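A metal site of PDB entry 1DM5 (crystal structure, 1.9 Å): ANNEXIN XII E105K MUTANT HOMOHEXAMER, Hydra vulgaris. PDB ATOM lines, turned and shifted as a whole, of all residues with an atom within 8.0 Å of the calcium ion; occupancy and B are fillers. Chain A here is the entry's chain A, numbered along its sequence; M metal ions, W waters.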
ATOM      1  N   ILE A 176      16.704  16.677 -20.593  1.00  0.00           N
ATOM      2  CA  ILE A 176      16.077  16.007 -21.735  1.00  0.00           C
ATOM      3  C   ILE A 176      16.753  16.425 -23.024  1.00  0.00           C
ATOM      4  O   ILE A 176      17.031  15.605 -23.908  1.00  0.00           O
ATOM      5  CB  ILE A 176      14.586  16.369 -21.767  1.00  0.00           C
ATOM      6  CG1 ILE A 176      13.805  15.821 -20.554  1.00  0.00           C
ATOM      7  CG2 ILE A 176      13.913  15.935 -23.052  1.00  0.00           C
ATOM      8  CD1 ILE A 176      12.339  16.225 -20.620  1.00  0.00           C
ATOM      9  N   TYR A 177      17.058  17.713 -23.175  1.00  0.00           N
ATOM     10  CA  TYR A 177      17.795  18.178 -24.352  1.00  0.00           C
ATOM     11  C   TYR A 177      19.136  17.461 -24.468  1.00  0.00           C
ATOM     12  O   TYR A 177      19.434  16.865 -25.505  1.00  0.00           O
ATOM     13  CB  TYR A 177      18.029  19.689 -24.256  1.00  0.00           C
ATOM     14  CG  TYR A 177      18.733  20.289 -25.454  1.00  0.00           C
ATOM     15  CD1 TYR A 177      17.992  20.696 -26.556  1.00  0.00           C
ATOM     16  CD2 TYR A 177      20.099  20.453 -25.479  1.00  0.00           C
ATOM     17  CE1 TYR A 177      18.594  21.247 -27.673  1.00  0.00           C
ATOM     18  CE2 TYR A 177      20.720  21.015 -26.586  1.00  0.00           C
ATOM     19  CZ  TYR A 177      19.962  21.413 -27.676  1.00  0.00           C
ATOM     20  OH  TYR A 177      20.575  21.969 -28.773  1.00  0.00           O
ATOM     21  N   GLN A 178      19.906  17.503 -23.387  1.00  0.00           N
ATOM     22  CA  GLN A 178      21.200  16.827 -23.337  1.00  0.00           C
ATOM     23  C   GLN A 178      21.063  15.325 -23.582  1.00  0.00           C
ATOM     24  O   GLN A 178      22.029  14.668 -23.973  1.00  0.00           O
ATOM     25  CB  GLN A 178      21.887  17.063 -21.995  1.00  0.00           C
ATOM     26  CG  GLN A 178      22.409  18.483 -21.820  1.00  0.00           C
ATOM     27  CD  GLN A 178      23.477  18.850 -22.846  1.00  0.00           C
ATOM     28  OE1 GLN A 178      23.301  19.807 -23.605  1.00  0.00           O
ATOM     29  NE2 GLN A 178      24.560  18.083 -22.869  1.00  0.00           N
ATOM     30  N   ALA A 179      19.876  14.807 -23.289  1.00  0.00           N
ATOM     31  CA  ALA A 179      19.548  13.403 -23.381  1.00  0.00           C
ATOM     32  C   ALA A 179      19.396  12.960 -24.827  1.00  0.00           C
ATOM     33  O   ALA A 179      19.580  11.792 -25.143  1.00  0.00           O
ATOM     34  CB  ALA A 179      18.251  13.102 -22.629  1.00  0.00           C
ATOM     35  N   GLY A 180      18.962  13.905 -25.664  1.00  0.00           N
ATOM     36  CA  GLY A 180      18.667  13.610 -27.048  1.00  0.00           C
ATOM     37  C   GLY A 180      19.414  14.546 -27.984  1.00  0.00           C
ATOM     38  O   GLY A 180      20.514  14.230 -28.414  1.00  0.00           O
ATOM     39  N   GLU A 181      18.837  15.708 -28.279  1.00  0.00           N
ATOM     40  CA  GLU A 181      19.467  16.657 -29.185  1.00  0.00           C
ATOM     41  C   GLU A 181      20.918  16.966 -28.808  1.00  0.00           C
ATOM     42  O   GLU A 181      21.795  17.090 -29.661  1.00  0.00           O
ATOM     43  CB  GLU A 181      18.678  17.958 -29.220  1.00  0.00           C
ATOM     44  CG  GLU A 181      17.310  17.891 -29.887  1.00  0.00           C
ATOM     45  CD  GLU A 181      16.735  19.284 -30.013  1.00  0.00           C
ATOM     46  OE1 GLU A 181      15.939  19.696 -29.139  1.00  0.00           O
ATOM     47  OE2 GLU A 181      17.183  19.995 -30.942  1.00  0.00           O
ATOM     48  N   GLY A 182      21.185  17.113 -27.514  1.00  0.00           N
ATOM     49  CA  GLY A 182      22.497  17.525 -27.070  1.00  0.00           C
ATOM     50  C   GLY A 182      23.643  16.606 -27.410  1.00  0.00           C
ATOM     51  O   GLY A 182      24.805  16.988 -27.258  1.00  0.00           O
ATOM     52  N   GLN A 183      23.353  15.394 -27.864  1.00  0.00           N
ATOM     53  CA  GLN A 183      24.396  14.384 -28.052  1.00  0.00           C
ATOM     54  C   GLN A 183      24.115  13.521 -29.262  1.00  0.00           C
ATOM     55  O   GLN A 183      23.027  13.567 -29.842  1.00  0.00           O
ATOM     56  CB  GLN A 183      24.514  13.527 -26.790  1.00  0.00           C
ATOM     57  CG  GLN A 183      23.252  12.703 -26.502  1.00  0.00           C
ATOM     58  CD  GLN A 183      23.508  11.608 -25.496  1.00  0.00           C
ATOM     59  OE1 GLN A 183      23.824  10.473 -25.861  1.00  0.00           O
ATOM     60  NE2 GLN A 183      23.367  11.918 -24.206  1.00  0.00           N
ATOM     61  N   ILE A 184      25.103  12.720 -29.667  1.00  0.00           N
ATOM     62  CA  ILE A 184      24.998  11.877 -30.843  1.00  0.00           C
ATOM     63  C   ILE A 184      24.063  10.687 -30.596  1.00  0.00           C
ATOM     64  O   ILE A 184      23.101  10.440 -31.329  1.00  0.00           O
ATOM     65  CB  ILE A 184      26.381  11.332 -31.243  1.00  0.00           C
ATOM     66  CG1 ILE A 184      27.370  12.403 -31.708  1.00  0.00           C
ATOM     67  CG2 ILE A 184      26.256  10.227 -32.282  1.00  0.00           C
ATOM     68  CD1 ILE A 184      27.439  12.561 -33.206  1.00  0.00           C
ATOM     69  N   GLY A 185      24.380   9.970 -29.522  1.00  0.00           N
ATOM     70  CA  GLY A 185      23.607   8.856 -29.034  1.00  0.00           C
ATOM     71  C   GLY A 185      22.459   9.349 -28.173  1.00  0.00           C
ATOM     72  O   GLY A 185      22.138  10.548 -28.152  1.00  0.00           O
ATOM     73  N   THR A 186      21.830   8.444 -27.425  1.00  0.00           N
ATOM     74  CA  THR A 186      20.673   8.872 -26.628  1.00  0.00           C
ATOM     75  C   THR A 186      20.782   8.417 -25.188  1.00  0.00           C
ATOM     76  O   THR A 186      21.538   7.488 -24.915  1.00  0.00           O
ATOM     77  CB  THR A 186      19.408   8.296 -27.293  1.00  0.00           C
ATOM     78  OG1 THR A 186      19.254   8.920 -28.576  1.00  0.00           O
ATOM     79  CG2 THR A 186      18.162   8.608 -26.485  1.00  0.00           C
ATOM     80  N   ASP A 187      20.117   9.104 -24.277  1.00  0.00           N
ATOM     81  CA  ASP A 187      19.870   8.653 -22.909  1.00  0.00           C
ATOM     82  C   ASP A 187      18.349   8.527 -22.750  1.00  0.00           C
ATOM     83  O   ASP A 187      17.725   9.359 -22.111  1.00  0.00           O
ATOM     84  CB  ASP A 187      20.414   9.601 -21.846  1.00  0.00           C
ATOM     85  CG  ASP A 187      20.245   9.045 -20.446  1.00  0.00           C
ATOM     86  OD1 ASP A 187      20.668   9.729 -19.493  1.00  0.00           O
ATOM     87  OD2 ASP A 187      19.683   7.940 -20.304  1.00  0.00           O
ATOM     88  N   GLU A 188      17.790   7.533 -23.415  1.00  0.00           N
ATOM     89  CA  GLU A 188      16.368   7.285 -23.462  1.00  0.00           C
ATOM     90  C   GLU A 188      15.763   7.261 -22.059  1.00  0.00           C
ATOM     91  O   GLU A 188      14.599   7.610 -21.831  1.00  0.00           O
ATOM     92  CB  GLU A 188      16.021   5.965 -24.149  1.00  0.00           C
ATOM     93  CG  GLU A 188      16.619   5.777 -25.528  1.00  0.00           C
ATOM     94  CD  GLU A 188      18.064   5.315 -25.522  1.00  0.00           C
ATOM     95  OE1 GLU A 188      18.269   4.085 -25.539  1.00  0.00           O
ATOM     96  OE2 GLU A 188      18.993   6.161 -25.534  1.00  0.00           O
ATOM     97  N   PHE A 191      14.294  10.503 -20.810  1.00  0.00           N
ATOM     98  CA  PHE A 191      12.973  10.802 -21.367  1.00  0.00           C
ATOM     99  C   PHE A 191      11.900  10.062 -20.571  1.00  0.00           C
ATOM    100  O   PHE A 191      10.849  10.598 -20.237  1.00  0.00           O
ATOM    101  CB  PHE A 191      12.889  10.407 -22.834  1.00  0.00           C
ATOM    102  CG  PHE A 191      13.524  11.429 -23.780  1.00  0.00           C
ATOM    103  CD1 PHE A 191      12.718  12.296 -24.497  1.00  0.00           C
ATOM    104  CD2 PHE A 191      14.893  11.509 -23.922  1.00  0.00           C
ATOM    105  CE1 PHE A 191      13.275  13.220 -25.364  1.00  0.00           C
ATOM    106  CE2 PHE A 191      15.467  12.409 -24.800  1.00  0.00           C
ATOM    107  CZ  PHE A 191      14.651  13.267 -25.530  1.00  0.00           C
ATOM    108  N   ALA A 221      11.465  16.831 -31.095  1.00  0.00           N
ATOM    109  CA  ALA A 221      12.703  16.171 -30.659  1.00  0.00           C
ATOM    110  C   ALA A 221      12.464  14.659 -30.516  1.00  0.00           C
ATOM    111  O   ALA A 221      13.226  13.840 -31.018  1.00  0.00           O
ATOM    112  CB  ALA A 221      13.182  16.766 -29.349  1.00  0.00           C
ATOM    113  N   ASN A 224      12.190  12.926 -33.577  1.00  0.00           N
ATOM    114  CA  ASN A 224      13.502  12.888 -34.171  1.00  0.00           C
ATOM    115  C   ASN A 224      14.431  11.866 -33.536  1.00  0.00           C
ATOM    116  O   ASN A 224      15.229  11.266 -34.250  1.00  0.00           O
ATOM    117  CB  ASN A 224      14.157  14.280 -34.112  1.00  0.00           C
ATOM    118  CG  ASN A 224      14.992  14.540 -35.351  1.00  0.00           C
ATOM    119  OD1 ASN A 224      14.516  15.166 -36.303  1.00  0.00           O
ATOM    120  ND2 ASN A 224      16.229  14.036 -35.347  1.00  0.00           N
ATOM    121  N   GLU A 225      14.325  11.728 -32.217  1.00  0.00           N
ATOM    122  CA  GLU A 225      15.186  10.891 -31.403  1.00  0.00           C
ATOM    123  C   GLU A 225      14.833   9.413 -31.440  1.00  0.00           C
ATOM    124  O   GLU A 225      15.701   8.569 -31.248  1.00  0.00           O
ATOM    125  CB  GLU A 225      15.153  11.358 -29.940  1.00  0.00           C
ATOM    126  CG  GLU A 225      16.390  11.011 -29.132  1.00  0.00           C
ATOM    127  CD  GLU A 225      17.665  11.616 -29.717  1.00  0.00           C
ATOM    128  OE1 GLU A 225      17.638  12.789 -30.150  1.00  0.00           O
ATOM    129  OE2 GLU A 225      18.680  10.892 -29.753  1.00  0.00           O
ATOM    130  N   PHE A 226      13.559   9.084 -31.603  1.00  0.00           N
ATOM    131  CA  PHE A 226      13.093   7.723 -31.400  1.00  0.00           C
ATOM    132  C   PHE A 226      12.272   7.228 -32.577  1.00  0.00           C
ATOM    133  O   PHE A 226      11.831   8.026 -33.411  1.00  0.00           O
ATOM    134  CB  PHE A 226      12.163   7.666 -30.175  1.00  0.00           C
ATOM    135  CG  PHE A 226      12.876   8.102 -28.898  1.00  0.00           C
ATOM    136  CD1 PHE A 226      13.866   7.292 -28.363  1.00  0.00           C
ATOM    137  CD2 PHE A 226      12.573   9.313 -28.303  1.00  0.00           C
ATOM    138  CE1 PHE A 226      14.568   7.705 -27.253  1.00  0.00           C
ATOM    139  CE2 PHE A 226      13.250   9.711 -27.171  1.00  0.00           C
ATOM    140  CZ  PHE A 226      14.238   8.904 -26.646  1.00  0.00           C
HETATM  141 CA    CA M   1      20.694  11.934 -29.586  1.00  0.00          CA
HETATM  142  O   HOH W   1      20.185  13.158 -31.575  1.00  0.00           O
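OE1 of Gln 183 lies within hydrogen-bond range of N of Thr 186.
NE2 of Gln 183 sits at hydrogen-bond distance from O of Gln 178, at 3.1 Å.
The backbone carbonyl oxygen (O) of Gly 185 sits close to the side-chain amide oxygen (OE1) of Gln 183, 2.8 Å away.
Ile 184 touches the calcium ion (O to CA, 3.3 Å).
Thr 186 touches the calcium ion.
The calcium ion is bound by the side-chain carboxylate (OE2) of Glu 225, at 2.3 Å.
Water W1 is bound to the calcium ion (2.4 Å).
The backbone carbonyl oxygen (O) of Gly 185 binds the calcium ion.
The calcium ion is bound by O of Gly 180 (2.6 Å).
The calcium ion is bound by O of Gln 183 (2.9 Å).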
